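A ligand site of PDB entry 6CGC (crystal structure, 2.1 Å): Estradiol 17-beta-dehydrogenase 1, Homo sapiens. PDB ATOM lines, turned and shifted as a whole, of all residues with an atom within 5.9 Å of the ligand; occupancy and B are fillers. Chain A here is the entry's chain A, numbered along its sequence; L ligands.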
ATOM      1  N   LEU A  94     -19.613  -5.897   8.879  1.00  0.00           N
ATOM      2  CA  LEU A  94     -20.806  -6.746   8.742  1.00  0.00           C
ATOM      3  C   LEU A  94     -21.212  -6.999   7.298  1.00  0.00           C
ATOM      4  O   LEU A  94     -21.038  -6.137   6.397  1.00  0.00           O
ATOM      5  CB  LEU A  94     -22.004  -6.097   9.456  1.00  0.00           C
ATOM      6  CG  LEU A  94     -21.772  -5.948  10.965  1.00  0.00           C
ATOM      7  CD1 LEU A  94     -22.929  -5.190  11.574  1.00  0.00           C
ATOM      8  CD2 LEU A  94     -21.648  -7.323  11.608  1.00  0.00           C
ATOM      9  N   GLY A  95     -21.771  -8.200   7.129  1.00  0.00           N
ATOM     10  CA  GLY A  95     -22.510  -8.587   5.956  1.00  0.00           C
ATOM     11  C   GLY A  95     -23.987  -8.345   6.092  1.00  0.00           C
ATOM     12  O   GLY A  95     -24.511  -8.132   7.189  1.00  0.00           O
ATOM     13  N   LEU A  96     -24.651  -8.291   4.953  1.00  0.00           N
ATOM     14  CA  LEU A  96     -26.105  -8.209   4.892  1.00  0.00           C
ATOM     15  C   LEU A  96     -26.518  -8.557   3.497  1.00  0.00           C
ATOM     16  O   LEU A  96     -26.104  -7.907   2.548  1.00  0.00           O
ATOM     17  CB  LEU A  96     -26.597  -6.809   5.217  1.00  0.00           C
ATOM     18  CG  LEU A  96     -28.063  -6.626   5.402  1.00  0.00           C
ATOM     19  CD1 LEU A  96     -28.570  -7.593   6.448  1.00  0.00           C
ATOM     20  CD2 LEU A  96     -28.321  -5.190   5.798  1.00  0.00           C
ATOM     21  N   LEU A  97     -27.360  -9.568   3.399  1.00  0.00           N
ATOM     22  CA  LEU A  97     -27.673 -10.211   2.169  1.00  0.00           C
ATOM     23  C   LEU A  97     -29.176 -10.428   2.076  1.00  0.00           C
ATOM     24  O   LEU A  97     -29.723 -11.164   2.850  1.00  0.00           O
ATOM     25  CB  LEU A  97     -26.967 -11.534   2.195  1.00  0.00           C
ATOM     26  CG  LEU A  97     -27.124 -12.437   0.993  1.00  0.00           C
ATOM     27  CD1 LEU A  97     -26.620 -11.752  -0.290  1.00  0.00           C
ATOM     28  CD2 LEU A  97     -26.363 -13.733   1.328  1.00  0.00           C
ATOM     29  N   SER A 143     -13.523  -4.813  -0.650  1.00  0.00           N
ATOM     30  CA  SER A 143     -14.159  -5.853  -1.406  1.00  0.00           C
ATOM     31  C   SER A 143     -14.283  -5.432  -2.851  1.00  0.00           C
ATOM     32  O   SER A 143     -14.413  -4.255  -3.193  1.00  0.00           O
ATOM     33  CB  SER A 143     -15.521  -6.172  -0.889  1.00  0.00           C
ATOM     34  OG  SER A 143     -16.131  -7.042  -1.813  1.00  0.00           O
ATOM     35  N   VAL A 144     -14.253  -6.433  -3.710  1.00  0.00           N
ATOM     36  CA  VAL A 144     -14.737  -6.250  -5.080  1.00  0.00           C
ATOM     37  C   VAL A 144     -16.208  -5.697  -5.160  1.00  0.00           C
ATOM     38  O   VAL A 144     -16.555  -4.955  -6.060  1.00  0.00           O
ATOM     39  CB  VAL A 144     -14.526  -7.575  -5.822  1.00  0.00           C
ATOM     40  CG1 VAL A 144     -15.375  -8.671  -5.186  1.00  0.00           C
ATOM     41  CG2 VAL A 144     -14.808  -7.456  -7.298  1.00  0.00           C
ATOM     42  N   GLY A 145     -17.029  -6.021  -4.151  1.00  0.00           N
ATOM     43  CA  GLY A 145     -18.320  -5.398  -3.892  1.00  0.00           C
ATOM     44  C   GLY A 145     -18.332  -3.903  -3.578  1.00  0.00           C
ATOM     45  O   GLY A 145     -19.386  -3.309  -3.540  1.00  0.00           O
ATOM     46  N   MET A 148     -17.916  -2.857  -7.688  1.00  0.00           N
ATOM     47  CA  MET A 148     -18.993  -3.110  -8.604  1.00  0.00           C
ATOM     48  C   MET A 148     -20.173  -3.583  -7.811  1.00  0.00           C
ATOM     49  O   MET A 148     -20.001  -4.238  -6.789  1.00  0.00           O
ATOM     50  CB  MET A 148     -18.569  -4.146  -9.621  1.00  0.00           C
ATOM     51  CG  MET A 148     -18.165  -5.498  -9.017  1.00  0.00           C
ATOM     52  SD  MET A 148     -17.527  -6.653 -10.266  1.00  0.00           S
ATOM     53  CE  MET A 148     -16.110  -5.767 -10.913  1.00  0.00           C
ATOM     54  N   LEU A 150     -23.498  -5.673  -6.768  1.00  0.00           N
ATOM     55  CA  LEU A 150     -24.114  -6.992  -6.955  1.00  0.00           C
ATOM     56  C   LEU A 150     -25.524  -7.177  -6.409  1.00  0.00           C
ATOM     57  O   LEU A 150     -25.839  -6.785  -5.281  1.00  0.00           O
ATOM     58  CB  LEU A 150     -23.221  -8.088  -6.405  1.00  0.00           C
ATOM     59  CG  LEU A 150     -22.148  -8.511  -7.421  1.00  0.00           C
ATOM     60  CD1 LEU A 150     -20.814  -7.834  -7.140  1.00  0.00           C
ATOM     61  CD2 LEU A 150     -22.064 -10.043  -7.471  1.00  0.00           C
ATOM     62  N   PHE A 152     -28.764  -8.124  -4.614  1.00  0.00           N
ATOM     63  CA  PHE A 152     -29.027  -8.610  -3.248  1.00  0.00           C
ATOM     64  C   PHE A 152     -27.921  -8.334  -2.271  1.00  0.00           C
ATOM     65  O   PHE A 152     -27.959  -8.857  -1.183  1.00  0.00           O
ATOM     66  CB  PHE A 152     -29.371 -10.104  -3.218  1.00  0.00           C
ATOM     67  CG  PHE A 152     -30.581 -10.435  -4.005  1.00  0.00           C
ATOM     68  CD1 PHE A 152     -31.838 -10.053  -3.519  1.00  0.00           C
ATOM     69  CD2 PHE A 152     -30.483 -11.029  -5.272  1.00  0.00           C
ATOM     70  CE1 PHE A 152     -32.993 -10.319  -4.233  1.00  0.00           C
ATOM     71  CE2 PHE A 152     -31.640 -11.317  -6.004  1.00  0.00           C
ATOM     72  CZ  PHE A 152     -32.896 -10.956  -5.491  1.00  0.00           C
ATOM     73  N   ASN A 153     -26.927  -7.530  -2.660  1.00  0.00           N
ATOM     74  CA  ASN A 153     -25.818  -7.117  -1.809  1.00  0.00           C
ATOM     75  C   ASN A 153     -25.823  -5.579  -1.796  1.00  0.00           C
ATOM     76  O   ASN A 153     -24.736  -4.967  -1.661  1.00  0.00           O
ATOM     77  CB  ASN A 153     -24.455  -7.574  -2.413  1.00  0.00           C
ATOM     78  CG  ASN A 153     -24.226  -9.081  -2.314  1.00  0.00           C
ATOM     79  OD1 ASN A 153     -23.613  -9.536  -1.350  1.00  0.00           O
ATOM     80  ND2 ASN A 153     -24.708  -9.836  -3.300  1.00  0.00           N
ATOM     81  N   TYR A 156     -24.641  -3.949   1.632  1.00  0.00           N
ATOM     82  CA  TYR A 156     -23.212  -4.347   1.772  1.00  0.00           C
ATOM     83  C   TYR A 156     -22.317  -3.593   0.766  1.00  0.00           C
ATOM     84  O   TYR A 156     -21.315  -2.911   1.193  1.00  0.00           O
ATOM     85  CB  TYR A 156     -23.010  -5.882   1.626  1.00  0.00           C
ATOM     86  CG  TYR A 156     -21.557  -6.329   1.644  1.00  0.00           C
ATOM     87  CD1 TYR A 156     -20.890  -6.571   2.824  1.00  0.00           C
ATOM     88  CD2 TYR A 156     -20.843  -6.469   0.419  1.00  0.00           C
ATOM     89  CE1 TYR A 156     -19.530  -6.942   2.834  1.00  0.00           C
ATOM     90  CE2 TYR A 156     -19.505  -6.842   0.399  1.00  0.00           C
ATOM     91  CZ  TYR A 156     -18.845  -7.102   1.602  1.00  0.00           C
ATOM     92  OH  TYR A 156     -17.518  -7.470   1.533  1.00  0.00           O
ATOM     93  N   CYS A 157     -22.697  -3.665  -0.510  1.00  0.00           N
ATOM     94  CA  CYS A 157     -22.054  -2.850  -1.559  1.00  0.00           C
ATOM     95  C   CYS A 157     -22.002  -1.355  -1.330  1.00  0.00           C
ATOM     96  O   CYS A 157     -20.960  -0.733  -1.542  1.00  0.00           O
ATOM     97  CB  CYS A 157     -22.648  -3.134  -2.938  1.00  0.00           C
ATOM     98  SG  CYS A 157     -22.295  -4.841  -3.491  1.00  0.00           S
ATOM     99  N   CYS A 186     -10.731  -7.703  -1.537  1.00  0.00           N
ATOM    100  CA  CYS A 186     -10.965  -9.138  -1.455  1.00  0.00           C
ATOM    101  C   CYS A 186     -12.101  -9.540  -2.363  1.00  0.00           C
ATOM    102  O   CYS A 186     -13.166  -8.910  -2.369  1.00  0.00           O
ATOM    103  CB  CYS A 186     -11.345  -9.567  -0.016  1.00  0.00           C
ATOM    104  SG  CYS A 186     -10.197  -9.002   1.298  1.00  0.00           S
ATOM    105  N   GLY A 187     -11.915 -10.622  -3.101  1.00  0.00           N
ATOM    106  CA  GLY A 187     -13.031 -11.301  -3.713  1.00  0.00           C
ATOM    107  C   GLY A 187     -13.753 -12.113  -2.673  1.00  0.00           C
ATOM    108  O   GLY A 187     -13.640 -11.863  -1.471  1.00  0.00           O
ATOM    109  N   PRO A 188     -14.481 -13.155  -3.114  1.00  0.00           N
ATOM    110  CA  PRO A 188     -15.024 -14.040  -2.089  1.00  0.00           C
ATOM    111  C   PRO A 188     -13.935 -14.676  -1.188  1.00  0.00           C
ATOM    112  O   PRO A 188     -12.885 -15.182  -1.684  1.00  0.00           O
ATOM    113  CB  PRO A 188     -15.839 -15.086  -2.879  1.00  0.00           C
ATOM    114  CG  PRO A 188     -15.475 -14.882  -4.321  1.00  0.00           C
ATOM    115  CD  PRO A 188     -14.787 -13.563  -4.488  1.00  0.00           C
ATOM    116  N   VAL A 189     -14.183 -14.607   0.121  1.00  0.00           N
ATOM    117  CA  VAL A 189     -13.387 -15.291   1.115  1.00  0.00           C
ATOM    118  C   VAL A 189     -14.173 -16.415   1.793  1.00  0.00           C
ATOM    119  O   VAL A 189     -15.275 -16.217   2.257  1.00  0.00           O
ATOM    120  CB  VAL A 189     -12.860 -14.355   2.201  1.00  0.00           C
ATOM    121  CG1 VAL A 189     -11.962 -15.110   3.162  1.00  0.00           C
ATOM    122  CG2 VAL A 189     -12.097 -13.208   1.565  1.00  0.00           C
ATOM    123  N   TYR A 219     -30.050 -16.361  -7.193  1.00  0.00           N
ATOM    124  CA  TYR A 219     -28.765 -15.704  -6.904  1.00  0.00           C
ATOM    125  C   TYR A 219     -27.943 -16.532  -5.902  1.00  0.00           C
ATOM    126  O   TYR A 219     -26.763 -16.750  -6.147  1.00  0.00           O
ATOM    127  CB  TYR A 219     -28.942 -14.258  -6.392  1.00  0.00           C
ATOM    128  CG  TYR A 219     -27.697 -13.769  -5.680  1.00  0.00           C
ATOM    129  CD1 TYR A 219     -26.639 -13.238  -6.412  1.00  0.00           C
ATOM    130  CD2 TYR A 219     -27.556 -13.903  -4.299  1.00  0.00           C
ATOM    131  CE1 TYR A 219     -25.465 -12.839  -5.785  1.00  0.00           C
ATOM    132  CE2 TYR A 219     -26.388 -13.489  -3.644  1.00  0.00           C
ATOM    133  CZ  TYR A 219     -25.344 -12.952  -4.394  1.00  0.00           C
ATOM    134  OH  TYR A 219     -24.179 -12.572  -3.765  1.00  0.00           O
ATOM    135  N   HIS A 222     -26.229 -19.532  -7.670  1.00  0.00           N
ATOM    136  CA  HIS A 222     -25.080 -19.145  -8.479  1.00  0.00           C
ATOM    137  C   HIS A 222     -23.933 -18.746  -7.545  1.00  0.00           C
ATOM    138  O   HIS A 222     -22.796 -19.185  -7.759  1.00  0.00           O
ATOM    139  CB  HIS A 222     -25.428 -18.029  -9.448  1.00  0.00           C
ATOM    140  CG  HIS A 222     -24.304 -17.701 -10.385  1.00  0.00           C
ATOM    141  ND1 HIS A 222     -23.986 -18.491 -11.472  1.00  0.00           N
ATOM    142  CD2 HIS A 222     -23.419 -16.679 -10.392  1.00  0.00           C
ATOM    143  CE1 HIS A 222     -22.955 -17.965 -12.104  1.00  0.00           C
ATOM    144  NE2 HIS A 222     -22.587 -16.859 -11.476  1.00  0.00           N
ATOM    145  N   SER A 223     -24.235 -17.944  -6.531  1.00  0.00           N
ATOM    146  CA  SER A 223     -23.258 -17.497  -5.520  1.00  0.00           C
ATOM    147  C   SER A 223     -22.433 -18.659  -4.916  1.00  0.00           C
ATOM    148  O   SER A 223     -21.203 -18.582  -4.886  1.00  0.00           O
ATOM    149  CB  SER A 223     -23.954 -16.727  -4.388  1.00  0.00           C
ATOM    150  OG  SER A 223     -22.995 -16.252  -3.465  1.00  0.00           O
ATOM    151  N   VAL A 226     -19.950 -19.774  -7.331  1.00  0.00           N
ATOM    152  CA  VAL A 226     -18.839 -18.852  -7.481  1.00  0.00           C
ATOM    153  C   VAL A 226     -17.893 -19.070  -6.309  1.00  0.00           C
ATOM    154  O   VAL A 226     -16.702 -19.170  -6.541  1.00  0.00           O
ATOM    155  CB  VAL A 226     -19.256 -17.379  -7.591  1.00  0.00           C
ATOM    156  CG1 VAL A 226     -18.024 -16.490  -7.699  1.00  0.00           C
ATOM    157  CG2 VAL A 226     -20.154 -17.162  -8.788  1.00  0.00           C
ATOM    158  N   PHE A 227     -18.428 -19.190  -5.081  1.00  0.00           N
ATOM    159  CA  PHE A 227     -17.626 -19.449  -3.846  1.00  0.00           C
ATOM    160  C   PHE A 227     -16.816 -20.767  -3.859  1.00  0.00           C
ATOM    161  O   PHE A 227     -15.642 -20.764  -3.508  1.00  0.00           O
ATOM    162  CB  PHE A 227     -18.481 -19.363  -2.555  1.00  0.00           C
ATOM    163  CG  PHE A 227     -18.535 -17.982  -1.960  1.00  0.00           C
ATOM    164  CD1 PHE A 227     -19.352 -16.999  -2.502  1.00  0.00           C
ATOM    165  CD2 PHE A 227     -17.771 -17.664  -0.829  1.00  0.00           C
ATOM    166  CE1 PHE A 227     -19.423 -15.722  -1.946  1.00  0.00           C
ATOM    167  CE2 PHE A 227     -17.820 -16.375  -0.257  1.00  0.00           C
ATOM    168  CZ  PHE A 227     -18.646 -15.399  -0.811  1.00  0.00           C
ATOM    169  N   PHE A 260     -11.506 -10.743 -11.104  1.00  0.00           N
ATOM    170  CA  PHE A 260     -12.621  -9.833 -11.417  1.00  0.00           C
ATOM    171  C   PHE A 260     -12.175  -8.608 -12.191  1.00  0.00           C
ATOM    172  O   PHE A 260     -13.010  -7.845 -12.628  1.00  0.00           O
ATOM    173  CB  PHE A 260     -13.417  -9.476 -10.116  1.00  0.00           C
ATOM    174  CG  PHE A 260     -13.889 -10.701  -9.362  1.00  0.00           C
ATOM    175  CD1 PHE A 260     -14.927 -11.512  -9.862  1.00  0.00           C
ATOM    176  CD2 PHE A 260     -13.244 -11.087  -8.172  1.00  0.00           C
ATOM    177  CE1 PHE A 260     -15.333 -12.670  -9.185  1.00  0.00           C
ATOM    178  CE2 PHE A 260     -13.643 -12.249  -7.513  1.00  0.00           C
ATOM    179  CZ  PHE A 260     -14.684 -13.036  -8.008  1.00  0.00           C
ATOM    180  N   LEU A 263     -14.264  -7.928 -15.666  1.00  0.00           N
ATOM    181  CA  LEU A 263     -15.540  -7.278 -15.386  1.00  0.00           C
ATOM    182  C   LEU A 263     -15.411  -5.834 -14.942  1.00  0.00           C
ATOM    183  O   LEU A 263     -16.162  -4.988 -15.375  1.00  0.00           O
ATOM    184  CB  LEU A 263     -16.287  -8.043 -14.300  1.00  0.00           C
ATOM    185  CG  LEU A 263     -17.258  -9.012 -14.938  1.00  0.00           C
ATOM    186  CD1 LEU A 263     -17.627 -10.067 -13.940  1.00  0.00           C
ATOM    187  CD2 LEU A 263     -18.485  -8.254 -15.436  1.00  0.00           C
ATOM    188  N   MET A 280     -23.506  -8.054 -15.939  1.00  0.00           N
ATOM    189  CA  MET A 280     -23.624  -8.608 -14.591  1.00  0.00           C
ATOM    190  C   MET A 280     -24.932  -9.360 -14.421  1.00  0.00           C
ATOM    191  O   MET A 280     -24.930 -10.448 -13.853  1.00  0.00           O
ATOM    192  CB  MET A 280     -23.437  -7.535 -13.490  1.00  0.00           C
ATOM    193  CG  MET A 280     -23.353  -8.081 -12.055  1.00  0.00           C
ATOM    194  SD  MET A 280     -22.225  -9.471 -11.723  1.00  0.00           S
ATOM    195  CE  MET A 280     -20.711  -8.832 -12.457  1.00  0.00           C
ATOM    196  N   GLU A 283     -24.348 -12.607 -16.286  1.00  0.00           N
ATOM    197  CA  GLU A 283     -23.371 -13.326 -15.455  1.00  0.00           C
ATOM    198  C   GLU A 283     -24.035 -14.015 -14.244  1.00  0.00           C
ATOM    199  O   GLU A 283     -23.842 -15.203 -14.018  1.00  0.00           O
ATOM    200  CB  GLU A 283     -22.276 -12.366 -15.008  1.00  0.00           C
ATOM    201  CG  GLU A 283     -21.059 -13.004 -14.375  1.00  0.00           C
ATOM    202  CD  GLU A 283     -20.199 -13.779 -15.356  1.00  0.00           C
ATOM    203  OE1 GLU A 283     -20.162 -15.019 -15.255  1.00  0.00           O
ATOM    204  OE2 GLU A 283     -19.560 -13.133 -16.229  1.00  0.00           O
ATOM    205  N   VAL A 284     -24.844 -13.271 -13.499  1.00  0.00           N
ATOM    206  CA  VAL A 284     -25.464 -13.794 -12.273  1.00  0.00           C
ATOM    207  C   VAL A 284     -26.631 -14.726 -12.568  1.00  0.00           C
ATOM    208  O   VAL A 284     -26.770 -15.745 -11.916  1.00  0.00           O
ATOM    209  CB  VAL A 284     -25.937 -12.649 -11.353  1.00  0.00           C
ATOM    210  CG1 VAL A 284     -26.772 -13.172 -10.177  1.00  0.00           C
ATOM    211  CG2 VAL A 284     -24.739 -11.857 -10.853  1.00  0.00           C
HETATM  212  O1  LIG L   1     -23.322  -9.585   3.203  1.00  0.00           O
HETATM  213  C1  LIG L   1     -23.038  -9.689   2.035  1.00  0.00           C
HETATM  214  N1  LIG L   1     -23.855  -9.169   1.132  1.00  0.00           N
HETATM  215  C2  LIG L   1     -21.737 -10.407   1.691  1.00  0.00           C
HETATM  216  C3  LIG L   1     -21.294 -11.472   2.510  1.00  0.00           C
HETATM  217  C4  LIG L   1     -20.081 -12.126   2.207  1.00  0.00           C
HETATM  218  C5  LIG L   1     -19.309 -11.738   1.111  1.00  0.00           C
HETATM  219  C6  LIG L   1     -19.740 -10.700   0.291  1.00  0.00           C
HETATM  220  C7  LIG L   1     -20.933 -10.033   0.589  1.00  0.00           C
HETATM  221  C8  LIG L   1     -18.897 -10.236  -0.880  1.00  0.00           C
HETATM  222  C9  LIG L   1     -18.515 -11.308  -1.894  1.00  0.00           C
HETATM  223  C10 LIG L   1     -17.575 -10.765  -2.969  1.00  0.00           C
HETATM  224  O2  LIG L   1     -16.989  -9.494  -2.641  1.00  0.00           O
HETATM  225  C11 LIG L   1     -18.388 -10.778  -4.260  1.00  0.00           C
HETATM  226  C12 LIG L   1     -19.317  -9.530  -4.366  1.00  0.00           C
HETATM  227  C13 LIG L   1     -19.112 -12.090  -4.065  1.00  0.00           C
HETATM  228  C14 LIG L   1     -19.688 -11.965  -2.642  1.00  0.00           C
HETATM  229  C15 LIG L   1     -17.547 -10.870  -5.555  1.00  0.00           C
HETATM  230  C16 LIG L   1     -18.240 -11.391  -6.803  1.00  0.00           C
HETATM  231  C17 LIG L   1     -19.107 -12.600  -6.509  1.00  0.00           C
HETATM  232  C18 LIG L   1     -19.904 -12.971  -7.697  1.00  0.00           C
HETATM  233  C19 LIG L   1     -21.217 -13.489  -7.545  1.00  0.00           C
HETATM  234  C20 LIG L   1     -21.934 -13.632  -6.208  1.00  0.00           C
HETATM  235  C21 LIG L   1     -21.020 -13.502  -4.990  1.00  0.00           C
HETATM  236  C22 LIG L   1     -20.018 -12.366  -5.260  1.00  0.00           C
HETATM  237  C23 LIG L   1     -21.946 -13.836  -8.679  1.00  0.00           C
HETATM  238  C24 LIG L   1     -21.378 -13.722  -9.959  1.00  0.00           C
HETATM  239  O3  LIG L   1     -22.037 -14.079 -11.097  1.00  0.00           O
HETATM  240  C25 LIG L   1     -20.094 -13.245 -10.113  1.00  0.00           C
HETATM  241  C26 LIG L   1     -19.337 -12.868  -8.986  1.00  0.00           C
HETATM  242  O4  LIG L   1     -19.571 -13.154 -11.395  1.00  0.00           O
HETATM  243  C27 LIG L   1     -18.978 -11.918 -11.766  1.00  0.00           C
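A nitrogen (N1) of the ligand sits at hydrogen-bond distance from the side-chain amide oxygen of Asn 153, 2.5 Å away.
An oxygen (O1) of the ligand is in hydrogen-bond range of the backbone NH (N) of Leu 96 (2.6 Å).
A nitrogen (N1) of the ligand sits at hydrogen-bond distance from the backbone carbonyl oxygen (O) of Leu 96.
OG of Ser 143 is in hydrogen-bond range of O2 of the ligand (2.7 Å).
A ring nitrogen (NE2) of His 222 lies within hydrogen-bond range of an oxygen (O3) of the ligand (2.9 Å).
The side-chain amide nitrogen of Asn 153 lies within hydrogen-bond range of the side-chain hydroxyl of Tyr 219.
The backbone carbonyl oxygen (O) of Asn 153 is in hydrogen-bond range of the side-chain sulfur (SG) of Cys 157.
The side-chain hydroxyl (OG) of Ser 143 lies within hydrogen-bond range of the backbone NH (N) of Gly 145 (2.7 Å).
A ring nitrogen (NE2) of His 222 sits at hydrogen-bond distance from the backbone carbonyl oxygen of Glu 283 (3.3 Å).
The backbone NH (N) of Val 144 is in hydrogen-bond range of the backbone carbonyl oxygen (O) of Cys 186 (3.0 Å).
N of Leu 150 sits at hydrogen-bond distance from SG of Cys 157 (3.6 Å).
The backbone carbonyl oxygen (O) of Gly 145 is in hydrogen-bond range of the side-chain sulfur (SG) of Cys 157, at 3.3 Å.
Gly 95 touches the ligand (CA to O1, 3.0 Å).
Val 144 touches the ligand.
N of Gly 145 touches O2 of the ligand, at 3.8 Å.
CD2 of Leu 150 touches C19 of the ligand, at 3.5 Å.
CB of Tyr 156 touches N1 of the ligand (3.4 Å).
Cys 186 touches the ligand.
Pro 188 touches the ligand (N to C10, 3.9 Å).
Tyr 219 touches the ligand.
OG of Ser 223 touches C21 of the ligand (3.7 Å).
CG2 of Val 226 touches C23 of the ligand (3.8 Å).
Phe 227 touches the ligand.
Phe 260 touches the ligand (CE1 to C16, 3.97 Å).
CD1 of Leu 263 touches C27 of the ligand, at 3.2 Å.
Met 280 touches the ligand (CE to C27, 3.6 Å).
Glu 283 touches the ligand (CG to O4, 3.3 Å).
Val 284 touches the ligand (CG2 to O3, 3.5 Å).
The nearest printed residue that does not touch the ligand is Leu 97 (4.04 Å).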
